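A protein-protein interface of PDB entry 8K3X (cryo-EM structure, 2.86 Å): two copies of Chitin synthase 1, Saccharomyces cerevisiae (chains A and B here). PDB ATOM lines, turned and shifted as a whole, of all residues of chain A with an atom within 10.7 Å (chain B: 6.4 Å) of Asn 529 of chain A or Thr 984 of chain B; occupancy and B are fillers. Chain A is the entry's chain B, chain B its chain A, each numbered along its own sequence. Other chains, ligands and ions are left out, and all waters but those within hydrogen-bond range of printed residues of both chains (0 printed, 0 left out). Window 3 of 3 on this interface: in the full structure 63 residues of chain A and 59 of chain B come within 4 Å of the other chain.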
ATOM      1  N   ASN A 382      14.530  14.829  15.497  1.00  0.00           N
ATOM      2  CA  ASN A 382      13.289  14.626  14.747  1.00  0.00           C
ATOM      3  C   ASN A 382      13.076  15.727  13.709  1.00  0.00           C
ATOM      4  O   ASN A 382      11.952  16.165  13.465  1.00  0.00           O
ATOM      5  CB  ASN A 382      12.086  14.527  15.684  1.00  0.00           C
ATOM      6  CG  ASN A 382      12.174  13.344  16.621  1.00  0.00           C
ATOM      7  OD1 ASN A 382      12.995  12.447  16.430  1.00  0.00           O
ATOM      8  ND2 ASN A 382      11.328  13.334  17.642  1.00  0.00           N
ATOM      9  N   GLY A 383      14.163  16.168  13.086  1.00  0.00           N
ATOM     10  CA  GLY A 383      14.098  17.257  12.136  1.00  0.00           C
ATOM     11  C   GLY A 383      14.082  18.634  12.754  1.00  0.00           C
ATOM     12  O   GLY A 383      13.991  19.624  12.017  1.00  0.00           O
ATOM     13  N   ASN A 384      14.176  18.733  14.076  1.00  0.00           N
ATOM     14  CA  ASN A 384      14.133  20.001  14.783  1.00  0.00           C
ATOM     15  C   ASN A 384      15.419  20.180  15.574  1.00  0.00           C
ATOM     16  O   ASN A 384      16.070  19.204  15.954  1.00  0.00           O
ATOM     17  CB  ASN A 384      12.924  20.062  15.720  1.00  0.00           C
ATOM     18  N   PHE A 385      15.784  21.434  15.817  1.00  0.00           N
ATOM     19  CA  PHE A 385      17.021  21.750  16.516  1.00  0.00           C
ATOM     20  C   PHE A 385      16.744  21.901  18.005  1.00  0.00           C
ATOM     21  O   PHE A 385      15.989  22.786  18.416  1.00  0.00           O
ATOM     22  CB  PHE A 385      17.649  23.025  15.957  1.00  0.00           C
ATOM     23  CG  PHE A 385      18.921  23.430  16.649  1.00  0.00           C
ATOM     24  CD1 PHE A 385      19.847  22.485  17.034  1.00  0.00           C
ATOM     25  CD2 PHE A 385      19.185  24.761  16.914  1.00  0.00           C
ATOM     26  CE1 PHE A 385      21.011  22.858  17.669  1.00  0.00           C
ATOM     27  CE2 PHE A 385      20.345  25.138  17.549  1.00  0.00           C
ATOM     28  CZ  PHE A 385      21.259  24.188  17.927  1.00  0.00           C
ATOM     29  N   VAL A 386      17.363  21.040  18.809  1.00  0.00           N
ATOM     30  CA  VAL A 386      17.338  21.150  20.258  1.00  0.00           C
ATOM     31  C   VAL A 386      18.777  21.102  20.751  1.00  0.00           C
ATOM     32  O   VAL A 386      19.679  20.620  20.063  1.00  0.00           O
ATOM     33  CB  VAL A 386      16.505  20.037  20.920  1.00  0.00           C
ATOM     34  CG1 VAL A 386      15.121  19.998  20.323  1.00  0.00           C
ATOM     35  CG2 VAL A 386      17.191  18.704  20.754  1.00  0.00           C
ATOM     36  N   ALA A 420      14.404  25.224  19.565  1.00  0.00           N
ATOM     37  CA  ALA A 420      14.139  26.467  18.815  1.00  0.00           C
ATOM     38  C   ALA A 420      12.925  26.244  17.927  1.00  0.00           C
ATOM     39  O   ALA A 420      13.015  25.402  17.032  1.00  0.00           O
ATOM     40  CB  ALA A 420      15.353  26.851  18.024  1.00  0.00           C
ATOM     41  N   THR A 422      10.184  27.282  15.053  1.00  0.00           N
ATOM     42  CA  THR A 422      10.204  28.101  13.821  1.00  0.00           C
ATOM     43  C   THR A 422       8.796  28.097  13.234  1.00  0.00           C
ATOM     44  O   THR A 422       8.488  29.017  12.462  1.00  0.00           O
ATOM     45  CB  THR A 422      11.210  27.479  12.854  1.00  0.00           C
ATOM     46  N   CYS A 423       7.971  27.127  13.611  1.00  0.00           N
ATOM     47  CA  CYS A 423       6.626  26.926  13.099  1.00  0.00           C
ATOM     48  C   CYS A 423       5.678  27.961  13.692  1.00  0.00           C
ATOM     49  O   CYS A 423       6.081  28.877  14.409  1.00  0.00           O
ATOM     50  CB  CYS A 423       6.150  25.510  13.409  1.00  0.00           C
ATOM     51  SG  CYS A 423       6.210  25.094  15.153  1.00  0.00           S
ATOM     52  N   LYS A 525      19.845  30.652  17.217  1.00  0.00           N
ATOM     53  CA  LYS A 525      20.045  30.389  15.793  1.00  0.00           C
ATOM     54  C   LYS A 525      18.929  31.037  14.992  1.00  0.00           C
ATOM     55  O   LYS A 525      17.799  30.542  14.974  1.00  0.00           O
ATOM     56  CB  LYS A 525      20.129  28.890  15.513  1.00  0.00           C
ATOM     57  CG  LYS A 525      21.345  28.250  16.151  1.00  0.00           C
ATOM     58  CD  LYS A 525      22.612  28.913  15.624  1.00  0.00           C
ATOM     59  CE  LYS A 525      23.855  28.416  16.332  1.00  0.00           C
ATOM     60  NZ  LYS A 525      23.955  28.947  17.712  1.00  0.00           N
ATOM     61  N   ASP A 526      19.267  32.118  14.300  1.00  0.00           N
ATOM     62  CA  ASP A 526      18.297  33.008  13.684  1.00  0.00           C
ATOM     63  C   ASP A 526      17.657  32.423  12.436  1.00  0.00           C
ATOM     64  O   ASP A 526      16.747  33.041  11.879  1.00  0.00           O
ATOM     65  CB  ASP A 526      18.972  34.333  13.360  1.00  0.00           C
ATOM     66  N   GLU A 527      18.126  31.270  11.977  1.00  0.00           N
ATOM     67  CA  GLU A 527      17.466  30.518  10.923  1.00  0.00           C
ATOM     68  C   GLU A 527      17.980  29.092  10.995  1.00  0.00           C
ATOM     69  O   GLU A 527      19.104  28.853  11.439  1.00  0.00           O
ATOM     70  CB  GLU A 527      17.724  31.114   9.537  1.00  0.00           C
ATOM     71  N   ILE A 528      17.148  28.148  10.572  1.00  0.00           N
ATOM     72  CA  ILE A 528      17.531  26.744  10.554  1.00  0.00           C
ATOM     73  C   ILE A 528      16.970  26.121   9.285  1.00  0.00           C
ATOM     74  O   ILE A 528      15.754  25.922   9.172  1.00  0.00           O
ATOM     75  CB  ILE A 528      17.052  25.991  11.799  1.00  0.00           C
ATOM     76  CG1 ILE A 528      17.961  26.330  12.976  1.00  0.00           C
ATOM     77  CG2 ILE A 528      17.047  24.491  11.561  1.00  0.00           C
ATOM     78  CD1 ILE A 528      17.296  26.232  14.306  1.00  0.00           C
ATOM     79  N   ASN A 529      17.848  25.840   8.321  1.00  0.00           N
ATOM     80  CA  ASN A 529      17.512  25.112   7.099  1.00  0.00           C
ATOM     81  C   ASN A 529      16.395  25.823   6.330  1.00  0.00           C
ATOM     82  O   ASN A 529      15.275  25.330   6.200  1.00  0.00           O
ATOM     83  CB  ASN A 529      17.135  23.664   7.425  1.00  0.00           C
ATOM     84  CG  ASN A 529      18.315  22.858   7.926  1.00  0.00           C
ATOM     85  OD1 ASN A 529      19.419  22.962   7.396  1.00  0.00           O
ATOM     86  ND2 ASN A 529      18.089  22.054   8.956  1.00  0.00           N
ATOM     87  N   GLU A 530      16.738  27.022   5.856  1.00  0.00           N
ATOM     88  CA  GLU A 530      15.867  27.879   5.040  1.00  0.00           C
ATOM     89  C   GLU A 530      14.524  28.171   5.720  1.00  0.00           C
ATOM     90  O   GLU A 530      13.554  28.563   5.063  1.00  0.00           O
ATOM     91  CB  GLU A 530      15.661  27.292   3.633  1.00  0.00           C
ATOM     92  N   LYS A 531      14.461  28.023   7.042  1.00  0.00           N
ATOM     93  CA  LYS A 531      13.263  28.307   7.820  1.00  0.00           C
ATOM     94  C   LYS A 531      13.621  29.298   8.916  1.00  0.00           C
ATOM     95  O   LYS A 531      14.514  29.031   9.725  1.00  0.00           O
ATOM     96  CB  LYS A 531      12.688  27.028   8.427  1.00  0.00           C
ATOM     97  CG  LYS A 531      11.965  26.147   7.434  1.00  0.00           C
ATOM     98  CD  LYS A 531      11.550  24.830   8.063  1.00  0.00           C
ATOM     99  CE  LYS A 531      10.915  23.919   7.032  1.00  0.00           C
ATOM    100  NZ  LYS A 531      10.677  22.558   7.579  1.00  0.00           N
ATOM    101  N   LYS A 532      12.926  30.428   8.944  1.00  0.00           N
ATOM    102  CA  LYS A 532      13.209  31.451   9.940  1.00  0.00           C
ATOM    103  C   LYS A 532      12.770  30.982  11.319  1.00  0.00           C
ATOM    104  O   LYS A 532      11.638  30.525  11.494  1.00  0.00           O
ATOM    105  CB  LYS A 532      12.497  32.751   9.579  1.00  0.00           C
ATOM    106  N   VAL A 533      13.658  31.107  12.304  1.00  0.00           N
ATOM    107  CA  VAL A 533      13.290  30.770  13.672  1.00  0.00           C
ATOM    108  C   VAL A 533      12.263  31.777  14.165  1.00  0.00           C
ATOM    109  O   VAL A 533      12.317  32.967  13.828  1.00  0.00           O
ATOM    110  CB  VAL A 533      14.523  30.741  14.589  1.00  0.00           C
ATOM    111  CG1 VAL A 533      15.031  32.135  14.843  1.00  0.00           C
ATOM    112  CG2 VAL A 533      14.195  30.064  15.891  1.00  0.00           C
ATOM    113  N   LYS B 981      23.221  30.885  12.050  1.00  0.00           N
ATOM    114  CA  LYS B 981      22.607  30.218  10.906  1.00  0.00           C
ATOM    115  C   LYS B 981      22.979  28.742  10.970  1.00  0.00           C
ATOM    116  O   LYS B 981      24.065  28.404  11.446  1.00  0.00           O
ATOM    117  CB  LYS B 981      23.074  30.841   9.588  1.00  0.00           C
ATOM    118  CG  LYS B 981      22.536  30.171   8.333  1.00  0.00           C
ATOM    119  CD  LYS B 981      21.073  30.509   8.114  1.00  0.00           C
ATOM    120  CE  LYS B 981      20.514  29.806   6.885  1.00  0.00           C
ATOM    121  NZ  LYS B 981      20.235  28.364   7.136  1.00  0.00           N
ATOM    122  N   ILE B 982      22.103  27.850  10.514  1.00  0.00           N
ATOM    123  CA  ILE B 982      22.416  26.425  10.494  1.00  0.00           C
ATOM    124  C   ILE B 982      21.916  25.823   9.188  1.00  0.00           C
ATOM    125  O   ILE B 982      20.712  25.850   8.906  1.00  0.00           O
ATOM    126  CB  ILE B 982      21.826  25.673  11.699  1.00  0.00           C
ATOM    127  N   ASN B 983      22.841  25.286   8.395  1.00  0.00           N
ATOM    128  CA  ASN B 983      22.537  24.527   7.191  1.00  0.00           C
ATOM    129  C   ASN B 983      23.119  23.132   7.353  1.00  0.00           C
ATOM    130  O   ASN B 983      24.301  22.987   7.683  1.00  0.00           O
ATOM    131  CB  ASN B 983      23.121  25.200   5.946  1.00  0.00           C
ATOM    132  N   THR B 984      22.293  22.112   7.141  1.00  0.00           N
ATOM    133  CA  THR B 984      22.724  20.729   7.269  1.00  0.00           C
ATOM    134  C   THR B 984      22.264  19.934   6.054  1.00  0.00           C
ATOM    135  O   THR B 984      21.499  20.418   5.215  1.00  0.00           O
ATOM    136  CB  THR B 984      22.193  20.077   8.554  1.00  0.00           C
ATOM    137  OG1 THR B 984      20.763  20.037   8.519  1.00  0.00           O
ATOM    138  CG2 THR B 984      22.650  20.851   9.781  1.00  0.00           C
ATOM    139  N   THR B 985      22.749  18.700   5.972  1.00  0.00           N
ATOM    140  CA  THR B 985      22.427  17.808   4.867  1.00  0.00           C
ATOM    141  C   THR B 985      21.091  17.119   5.138  1.00  0.00           C
ATOM    142  O   THR B 985      20.393  17.424   6.109  1.00  0.00           O
ATOM    143  CB  THR B 985      23.554  16.802   4.661  1.00  0.00           C
ATOM    144  OG1 THR B 985      23.585  15.893   5.767  1.00  0.00           O
ATOM    145  CG2 THR B 985      24.889  17.522   4.571  1.00  0.00           C
ATOM    146  N   GLU B 986      20.723  16.168   4.275  1.00  0.00           N
ATOM    147  CA  GLU B 986      19.474  15.438   4.468  1.00  0.00           C
ATOM    148  C   GLU B 986      19.491  14.654   5.773  1.00  0.00           C
ATOM    149  O   GLU B 986      18.469  14.557   6.462  1.00  0.00           O
ATOM    150  CB  GLU B 986      19.215  14.515   3.276  1.00  0.00           C
ATOM    151  CG  GLU B 986      20.340  13.533   2.973  1.00  0.00           C
ATOM    152  CD  GLU B 986      20.168  12.198   3.672  1.00  0.00           C
ATOM    153  OE1 GLU B 986      19.029  11.869   4.064  1.00  0.00           O
ATOM    154  OE2 GLU B 986      21.175  11.476   3.829  1.00  0.00           O
ATOM    155  N   ASP B 987      20.644  14.087   6.129  1.00  0.00           N
ATOM    156  CA  ASP B 987      20.770  13.407   7.413  1.00  0.00           C
ATOM    157  C   ASP B 987      20.594  14.385   8.569  1.00  0.00           C
ATOM    158  O   ASP B 987      19.933  14.071   9.565  1.00  0.00           O
ATOM    159  CB  ASP B 987      22.127  12.704   7.496  1.00  0.00           C
ATOM    160  CG  ASP B 987      22.300  11.918   8.776  1.00  0.00           C
ATOM    161  OD1 ASP B 987      21.854  10.752   8.826  1.00  0.00           O
ATOM    162  OD2 ASP B 987      22.885  12.464   9.733  1.00  0.00           O
ATOM    163  N   GLY B 988      21.171  15.579   8.447  1.00  0.00           N
ATOM    164  CA  GLY B 988      21.080  16.581   9.489  1.00  0.00           C
ATOM    165  C   GLY B 988      22.228  16.543  10.477  1.00  0.00           C
ATOM    166  O   GLY B 988      22.007  16.481  11.690  1.00  0.00           O
ATOM    167  N   THR B 989      23.458  16.574   9.976  1.00  0.00           N
ATOM    168  CA  THR B 989      24.642  16.576  10.821  1.00  0.00           C
ATOM    169  C   THR B 989      25.556  17.716  10.401  1.00  0.00           C
ATOM    170  O   THR B 989      25.746  17.965   9.207  1.00  0.00           O
ATOM    171  CB  THR B 989      25.388  15.237  10.742  1.00  0.00           C
ATOM    172  N   PHE B 990      26.109  18.407  11.391  1.00  0.00           N
ATOM    173  CA  PHE B 990      26.998  19.539  11.163  1.00  0.00           C
ATOM    174  C   PHE B 990      27.636  19.868  12.507  1.00  0.00           C
ATOM    175  O   PHE B 990      27.296  19.271  13.532  1.00  0.00           O
ATOM    176  CB  PHE B 990      26.231  20.725  10.577  1.00  0.00           C
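The backbone NH (N) of Asn 529 of chain A is in hydrogen-bond range of the backbone carbonyl oxygen (O) of Ile 982 of chain B (2.9 Å). The side-chain amide oxygen of Asn 529 of chain A is in hydrogen-bond range of the backbone NH of Thr 984 of chain B, at 3.0 Å. N of Ile 982 of chain B is in hydrogen-bond range of O of Glu 527 of chain A (3.3 Å).
Among the printed residues, merely in contact across the chains: Glu 527 of chain A with Lys 981 of chain B (3.7 Å), Ile 528 of chain A with Ile 982 of chain B (3.7 Å), Asn 529 of chain A with Lys 981 of chain B (3.7 Å), Asn 529 of chain A with Asn 983 of chain B (3.5 Å) and Glu 530 of chain A with Lys 981 of chain B (3.96 Å).
Of chain B, only Lys 981, Ile 982, Asn 983 and Thr 984 come within 4 Å of Asn 529 of chain A. Thr 984 of chain B touches one residue of chain A. Ile 982 of chain B touches just these residues of chain A: Glu 527, Ile 528 and Asn 529. Of chain A, only Asn 529 (3.5 Å) comes within 4 Å of Asn 983 of chain B. No residue of chain A comes within 4 Å of Thr 985 of chain B. No residue of chain A comes within 4 Å of Gly 988 of chain B. No residue of chain A comes within 4 Å of Thr 989 of chain B. Printed residues of chain B within 4 Å of Glu 527 of chain A: Lys 981 and Ile 982. Printed residues of chain B within 4 Å of Ile 528 of chain A: Ile 982 (3.7 Å). Printed residues of chain A within 4 Å of Lys 981 of chain B: Glu 527, Asn 529 and Glu 530. The nearest residue of chain B that does not touch Asn 529 of chain A is Thr 985 of chain B (5.6 Å).
Of the 17 printed residues of chain A, 4 touch a printed residue of chain B. Among the printed residues, 8 pairs touch across the chains. Among the printed residues, no Asp or Glu carboxylate lies within 4 Å of a Lys or Arg side-chain nitrogen of the other chain.
No position is printed for both chains. Of the 8 pairs that touch across the chains among the printed residues, none has its exchanged pair printed and touching as well.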
